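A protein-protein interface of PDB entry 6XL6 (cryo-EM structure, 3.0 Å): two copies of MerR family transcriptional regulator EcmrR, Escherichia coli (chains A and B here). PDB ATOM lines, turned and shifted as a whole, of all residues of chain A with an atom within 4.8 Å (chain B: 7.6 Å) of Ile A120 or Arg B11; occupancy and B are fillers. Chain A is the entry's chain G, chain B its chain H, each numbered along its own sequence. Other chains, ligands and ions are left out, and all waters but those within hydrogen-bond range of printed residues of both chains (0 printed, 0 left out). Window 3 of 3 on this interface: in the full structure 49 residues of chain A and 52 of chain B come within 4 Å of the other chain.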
ATOM      1  N   LYS A 118      23.018  11.429  -5.078  1.00  0.00           N
ATOM      2  CA  LYS A 118      23.532  11.587  -6.429  1.00  0.00           C
ATOM      3  C   LYS A 118      24.268  10.330  -6.862  1.00  0.00           C
ATOM      4  O   LYS A 118      24.848   9.621  -6.036  1.00  0.00           O
ATOM      5  CB  LYS A 118      24.459  12.802  -6.537  1.00  0.00           C
ATOM      6  CG  LYS A 118      25.713  12.720  -5.694  1.00  0.00           C
ATOM      7  CD  LYS A 118      26.482  14.028  -5.749  1.00  0.00           C
ATOM      8  CE  LYS A 118      25.599  15.201  -5.340  1.00  0.00           C
ATOM      9  NZ  LYS A 118      26.308  16.506  -5.433  1.00  0.00           N
ATOM     10  N   GLU A 119      24.233  10.059  -8.163  1.00  0.00           N
ATOM     11  CA  GLU A 119      24.837   8.862  -8.733  1.00  0.00           C
ATOM     12  C   GLU A 119      26.232   9.191  -9.242  1.00  0.00           C
ATOM     13  O   GLU A 119      26.404  10.113 -10.046  1.00  0.00           O
ATOM     14  CB  GLU A 119      23.975   8.309  -9.865  1.00  0.00           C
ATOM     15  CG  GLU A 119      22.606   7.836  -9.428  1.00  0.00           C
ATOM     16  CD  GLU A 119      21.916   7.017 -10.496  1.00  0.00           C
ATOM     17  OE1 GLU A 119      22.463   5.966 -10.886  1.00  0.00           O
ATOM     18  OE2 GLU A 119      20.829   7.429 -10.951  1.00  0.00           O
ATOM     19  N   ILE A 120      27.220   8.431  -8.789  1.00  0.00           N
ATOM     20  CA  ILE A 120      28.616   8.635  -9.163  1.00  0.00           C
ATOM     21  C   ILE A 120      28.979   7.586 -10.208  1.00  0.00           C
ATOM     22  O   ILE A 120      28.828   6.387  -9.937  1.00  0.00           O
ATOM     23  CB  ILE A 120      29.544   8.539  -7.946  1.00  0.00           C
ATOM     24  CG1 ILE A 120      28.999   9.386  -6.801  1.00  0.00           C
ATOM     25  CG2 ILE A 120      30.938   8.992  -8.314  1.00  0.00           C
ATOM     26  CD1 ILE A 120      29.723   9.176  -5.509  1.00  0.00           C
ATOM     27  N   PRO A 121      29.452   7.980 -11.389  1.00  0.00           N
ATOM     28  CA  PRO A 121      29.807   6.988 -12.407  1.00  0.00           C
ATOM     29  C   PRO A 121      31.070   6.235 -12.021  1.00  0.00           C
ATOM     30  O   PRO A 121      31.816   6.636 -11.126  1.00  0.00           O
ATOM     31  CB  PRO A 121      30.028   7.831 -13.669  1.00  0.00           C
ATOM     32  CG  PRO A 121      29.546   9.216 -13.326  1.00  0.00           C
ATOM     33  CD  PRO A 121      29.688   9.352 -11.855  1.00  0.00           C
ATOM     34  N   GLU A 122      31.303   5.124 -12.712  1.00  0.00           N
ATOM     35  CA  GLU A 122      32.513   4.352 -12.478  1.00  0.00           C
ATOM     36  C   GLU A 122      33.726   5.116 -12.990  1.00  0.00           C
ATOM     37  O   GLU A 122      33.622   5.990 -13.855  1.00  0.00           O
ATOM     38  CB  GLU A 122      32.422   2.986 -13.153  1.00  0.00           C
ATOM     39  CG  GLU A 122      32.283   3.048 -14.659  1.00  0.00           C
ATOM     40  CD  GLU A 122      32.468   1.695 -15.316  1.00  0.00           C
ATOM     41  OE1 GLU A 122      33.060   0.801 -14.675  1.00  0.00           O
ATOM     42  OE2 GLU A 122      32.024   1.527 -16.470  1.00  0.00           O
ATOM     43  N   TYR A 163      38.583  13.686  -9.480  1.00  0.00           N
ATOM     44  CA  TYR A 163      37.907  12.888  -8.461  1.00  0.00           C
ATOM     45  C   TYR A 163      38.981  12.218  -7.617  1.00  0.00           C
ATOM     46  O   TYR A 163      39.531  11.179  -7.978  1.00  0.00           O
ATOM     47  CB  TYR A 163      36.968  11.877  -9.105  1.00  0.00           C
ATOM     48  CG  TYR A 163      36.092  11.133  -8.129  1.00  0.00           C
ATOM     49  CD1 TYR A 163      35.744  11.689  -6.912  1.00  0.00           C
ATOM     50  CD2 TYR A 163      35.606   9.873  -8.433  1.00  0.00           C
ATOM     51  CE1 TYR A 163      34.945  11.012  -6.026  1.00  0.00           C
ATOM     52  CE2 TYR A 163      34.807   9.189  -7.552  1.00  0.00           C
ATOM     53  CZ  TYR A 163      34.479   9.760  -6.351  1.00  0.00           C
ATOM     54  OH  TYR A 163      33.679   9.078  -5.471  1.00  0.00           O
ATOM     55  N   ALA A 203      30.390   2.090 -10.120  1.00  0.00           N
ATOM     56  CA  ALA A 203      29.464   3.206 -10.018  1.00  0.00           C
ATOM     57  C   ALA A 203      28.480   2.971  -8.882  1.00  0.00           C
ATOM     58  O   ALA A 203      27.902   1.889  -8.752  1.00  0.00           O
ATOM     59  CB  ALA A 203      28.717   3.397 -11.336  1.00  0.00           C
ATOM     60  N   ILE A 204      28.289   3.996  -8.056  1.00  0.00           N
ATOM     61  CA  ILE A 204      27.489   3.887  -6.844  1.00  0.00           C
ATOM     62  C   ILE A 204      26.456   5.002  -6.813  1.00  0.00           C
ATOM     63  O   ILE A 204      26.698   6.107  -7.308  1.00  0.00           O
ATOM     64  CB  ILE A 204      28.365   3.945  -5.579  1.00  0.00           C
ATOM     65  CG1 ILE A 204      29.226   5.207  -5.597  1.00  0.00           C
ATOM     66  CG2 ILE A 204      29.226   2.704  -5.468  1.00  0.00           C
ATOM     67  CD1 ILE A 204      29.600   5.702  -4.231  1.00  0.00           C
ATOM     68  N   ALA A 206      24.975   7.334  -4.116  1.00  0.00           N
ATOM     69  CA  ALA A 206      25.449   7.731  -2.802  1.00  0.00           C
ATOM     70  C   ALA A 206      24.756   8.998  -2.334  1.00  0.00           C
ATOM     71  O   ALA A 206      24.553   9.938  -3.108  1.00  0.00           O
ATOM     72  CB  ALA A 206      26.961   7.950  -2.808  1.00  0.00           C
ATOM     73  N   ARG A 241      33.153   7.222   1.040  1.00  0.00           N
ATOM     74  CA  ARG A 241      34.189   7.968   0.347  1.00  0.00           C
ATOM     75  C   ARG A 241      34.252   9.388   0.885  1.00  0.00           C
ATOM     76  O   ARG A 241      33.278   9.908   1.432  1.00  0.00           O
ATOM     77  CB  ARG A 241      33.933   8.006  -1.159  1.00  0.00           C
ATOM     78  CG  ARG A 241      33.415   6.712  -1.729  1.00  0.00           C
ATOM     79  CD  ARG A 241      33.475   6.742  -3.235  1.00  0.00           C
ATOM     80  NE  ARG A 241      32.995   5.503  -3.825  1.00  0.00           N
ATOM     81  CZ  ARG A 241      32.920   5.289  -5.131  1.00  0.00           C
ATOM     82  NH1 ARG A 241      33.293   6.237  -5.976  1.00  0.00           N
ATOM     83  NH2 ARG A 241      32.466   4.134  -5.590  1.00  0.00           N
ATOM     84  N   GLN A 262      30.758  10.896   0.838  1.00  0.00           N
ATOM     85  CA  GLN A 262      29.837  10.118   0.020  1.00  0.00           C
ATOM     86  C   GLN A 262      29.596   8.773   0.685  1.00  0.00           C
ATOM     87  O   GLN A 262      30.548   8.082   1.059  1.00  0.00           O
ATOM     88  CB  GLN A 262      30.392   9.939  -1.391  1.00  0.00           C
ATOM     89  CG  GLN A 262      30.724  11.252  -2.068  1.00  0.00           C
ATOM     90  CD  GLN A 262      31.632  11.084  -3.258  1.00  0.00           C
ATOM     91  OE1 GLN A 262      32.440  10.160  -3.309  1.00  0.00           O
ATOM     92  NE2 GLN A 262      31.501  11.975  -4.229  1.00  0.00           N
ATOM     93  N   LEU B   5      33.099  22.646 -17.336  1.00  0.00           N
ATOM     94  CA  LEU B   5      33.770  21.979 -16.227  1.00  0.00           C
ATOM     95  C   LEU B   5      32.889  21.952 -14.988  1.00  0.00           C
ATOM     96  O   LEU B   5      32.781  20.919 -14.321  1.00  0.00           O
ATOM     97  CB  LEU B   5      35.096  22.669 -15.923  1.00  0.00           C
ATOM     98  CG  LEU B   5      35.940  21.962 -14.870  1.00  0.00           C
ATOM     99  CD1 LEU B   5      36.205  20.531 -15.296  1.00  0.00           C
ATOM    100  CD2 LEU B   5      37.240  22.709 -14.637  1.00  0.00           C
ATOM    101  N   PHE B   6      32.247  23.078 -14.669  1.00  0.00           N
ATOM    102  CA  PHE B   6      31.354  23.111 -13.519  1.00  0.00           C
ATOM    103  C   PHE B   6      30.158  22.195 -13.721  1.00  0.00           C
ATOM    104  O   PHE B   6      29.721  21.521 -12.783  1.00  0.00           O
ATOM    105  CB  PHE B   6      30.885  24.536 -13.250  1.00  0.00           C
ATOM    106  CG  PHE B   6      30.214  24.705 -11.925  1.00  0.00           C
ATOM    107  CD1 PHE B   6      30.939  24.606 -10.752  1.00  0.00           C
ATOM    108  CD2 PHE B   6      28.856  24.953 -11.847  1.00  0.00           C
ATOM    109  CE1 PHE B   6      30.326  24.758  -9.534  1.00  0.00           C
ATOM    110  CE2 PHE B   6      28.239  25.105 -10.630  1.00  0.00           C
ATOM    111  CZ  PHE B   6      28.972  25.008  -9.474  1.00  0.00           C
ATOM    112  N   SER B   7      29.613  22.153 -14.939  1.00  0.00           N
ATOM    113  CA  SER B   7      28.497  21.256 -15.204  1.00  0.00           C
ATOM    114  C   SER B   7      28.918  19.799 -15.104  1.00  0.00           C
ATOM    115  O   SER B   7      28.097  18.937 -14.774  1.00  0.00           O
ATOM    116  CB  SER B   7      27.906  21.547 -16.579  1.00  0.00           C
ATOM    117  OG  SER B   7      28.825  21.233 -17.606  1.00  0.00           O
ATOM    118  N   LYS B   8      30.187  19.502 -15.384  1.00  0.00           N
ATOM    119  CA  LYS B   8      30.687  18.147 -15.183  1.00  0.00           C
ATOM    120  C   LYS B   8      30.928  17.842 -13.711  1.00  0.00           C
ATOM    121  O   LYS B   8      30.807  16.685 -13.297  1.00  0.00           O
ATOM    122  CB  LYS B   8      31.976  17.936 -15.974  1.00  0.00           C
ATOM    123  CG  LYS B   8      31.764  17.689 -17.454  1.00  0.00           C
ATOM    124  CD  LYS B   8      33.029  17.162 -18.101  1.00  0.00           C
ATOM    125  CE  LYS B   8      32.793  16.780 -19.551  1.00  0.00           C
ATOM    126  NZ  LYS B   8      34.009  16.184 -20.170  1.00  0.00           N
ATOM    127  N   ILE B   9      31.283  18.855 -12.918  1.00  0.00           N
ATOM    128  CA  ILE B   9      31.470  18.650 -11.482  1.00  0.00           C
ATOM    129  C   ILE B   9      30.153  18.249 -10.832  1.00  0.00           C
ATOM    130  O   ILE B   9      30.076  17.265 -10.089  1.00  0.00           O
ATOM    131  CB  ILE B   9      32.044  19.918 -10.827  1.00  0.00           C
ATOM    132  CG1 ILE B   9      33.470  20.176 -11.300  1.00  0.00           C
ATOM    133  CG2 ILE B   9      32.007  19.795  -9.319  1.00  0.00           C
ATOM    134  CD1 ILE B   9      34.098  21.410 -10.702  1.00  0.00           C
ATOM    135  N   CYS B  10      29.096  19.010 -11.114  1.00  0.00           N
ATOM    136  CA  CYS B  10      27.814  18.784 -10.461  1.00  0.00           C
ATOM    137  C   CYS B  10      27.030  17.651 -11.110  1.00  0.00           C
ATOM    138  O   CYS B  10      25.981  17.258 -10.587  1.00  0.00           O
ATOM    139  CB  CYS B  10      26.995  20.071 -10.487  1.00  0.00           C
ATOM    140  SG  CYS B  10      27.935  21.568 -10.141  1.00  0.00           S
ATOM    141  N   ARG B  11      27.520  17.120 -12.232  1.00  0.00           N
ATOM    142  CA  ARG B  11      26.798  16.131 -13.038  1.00  0.00           C
ATOM    143  C   ARG B  11      25.425  16.662 -13.445  1.00  0.00           C
ATOM    144  O   ARG B  11      24.394  16.028 -13.216  1.00  0.00           O
ATOM    145  CB  ARG B  11      26.670  14.792 -12.308  1.00  0.00           C
ATOM    146  CG  ARG B  11      27.982  14.110 -11.992  1.00  0.00           C
ATOM    147  CD  ARG B  11      27.847  13.240 -10.752  1.00  0.00           C
ATOM    148  NE  ARG B  11      29.039  12.436 -10.513  1.00  0.00           N
ATOM    149  CZ  ARG B  11      30.150  12.896  -9.949  1.00  0.00           C
ATOM    150  NH1 ARG B  11      30.223  14.161  -9.560  1.00  0.00           N
ATOM    151  NH2 ARG B  11      31.188  12.091  -9.772  1.00  0.00           N
ATOM    152  N   VAL B  12      25.418  17.849 -14.054  1.00  0.00           N
ATOM    153  CA  VAL B  12      24.183  18.521 -14.432  1.00  0.00           C
ATOM    154  C   VAL B  12      24.369  19.108 -15.826  1.00  0.00           C
ATOM    155  O   VAL B  12      25.487  19.233 -16.329  1.00  0.00           O
ATOM    156  CB  VAL B  12      23.799  19.617 -13.411  1.00  0.00           C
ATOM    157  CG1 VAL B  12      24.659  20.858 -13.594  1.00  0.00           C
ATOM    158  CG2 VAL B  12      22.314  19.928 -13.456  1.00  0.00           C
ATOM    159  N   THR B  13      23.253  19.460 -16.457  1.00  0.00           N
ATOM    160  CA  THR B  13      23.284  19.978 -17.816  1.00  0.00           C
ATOM    161  C   THR B  13      23.712  21.440 -17.822  1.00  0.00           C
ATOM    162  O   THR B  13      23.514  22.164 -16.843  1.00  0.00           O
ATOM    163  CB  THR B  13      21.907  19.831 -18.459  1.00  0.00           C
ATOM    164  OG1 THR B  13      21.333  18.580 -18.065  1.00  0.00           O
ATOM    165  CG2 THR B  13      22.013  19.858 -19.973  1.00  0.00           C
ATOM    166  N   LEU B  45      29.541  25.492  -6.066  1.00  0.00           N
ATOM    167  CA  LEU B  45      29.297  24.058  -5.963  1.00  0.00           C
ATOM    168  C   LEU B  45      28.557  23.722  -4.676  1.00  0.00           C
ATOM    169  O   LEU B  45      27.626  22.907  -4.682  1.00  0.00           O
ATOM    170  CB  LEU B  45      30.617  23.294  -6.043  1.00  0.00           C
ATOM    171  CG  LEU B  45      30.564  21.800  -5.731  1.00  0.00           C
ATOM    172  CD1 LEU B  45      29.592  21.093  -6.657  1.00  0.00           C
ATOM    173  CD2 LEU B  45      31.945  21.189  -5.843  1.00  0.00           C
ATOM    174  N   PHE B  48      24.967  24.720  -5.270  1.00  0.00           N
ATOM    175  CA  PHE B  48      24.241  23.774  -6.108  1.00  0.00           C
ATOM    176  C   PHE B  48      23.949  22.490  -5.350  1.00  0.00           C
ATOM    177  O   PHE B  48      22.954  21.815  -5.630  1.00  0.00           O
ATOM    178  CB  PHE B  48      25.016  23.463  -7.386  1.00  0.00           C
ATOM    179  CG  PHE B  48      24.292  22.520  -8.304  1.00  0.00           C
ATOM    180  CD1 PHE B  48      23.363  22.995  -9.206  1.00  0.00           C
ATOM    181  CD2 PHE B  48      24.517  21.156  -8.243  1.00  0.00           C
ATOM    182  CE1 PHE B  48      22.687  22.132 -10.037  1.00  0.00           C
ATOM    183  CE2 PHE B  48      23.836  20.290  -9.067  1.00  0.00           C
ATOM    184  CZ  PHE B  48      22.926  20.777  -9.967  1.00  0.00           C
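The backbone NH of Ile A120 sits at hydrogen-bond distance from the backbone carbonyl oxygen of Ile A204 (2.8 Å). O of Ile B9 sits at hydrogen-bond distance from NH1 of Arg B11, 3.2 Å away.
Glu A119 touches Arg B11 (O to CD, 3.5 Å). Ile A120 touches Arg B11. CD of Pro A121 touches NE of Arg B11, at 3.4 Å.
Of the printed residues of chain B, Ile A120 touches Arg B11 (3.4 Å). Of chain A, only Glu A119 (3.5 Å), Ile A120 (3.4 Å) and Pro A121 (3.4 Å) come within 4 Å of Arg B11. Of the printed residues of chain B, Pro A121 touches Arg B11. Of the printed residues of chain B, Glu A119 touches Arg B11 (3.5 Å). Cys B10 touches none of the printed residues of chain A. Ile B9 touches none of the printed residues of chain A. The nearest printed residue of chain B that does not touch Glu A119 is Cys B10 (7.2 Å).
Printed residues of chain B that touch a printed residue of chain A: Arg B11. Among the printed residues, 3 pairs touch across the chains.
No position is printed for both chains. Of the 3 pairs that touch across the chains among the printed residues, none has its exchanged pair printed and touching as well.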
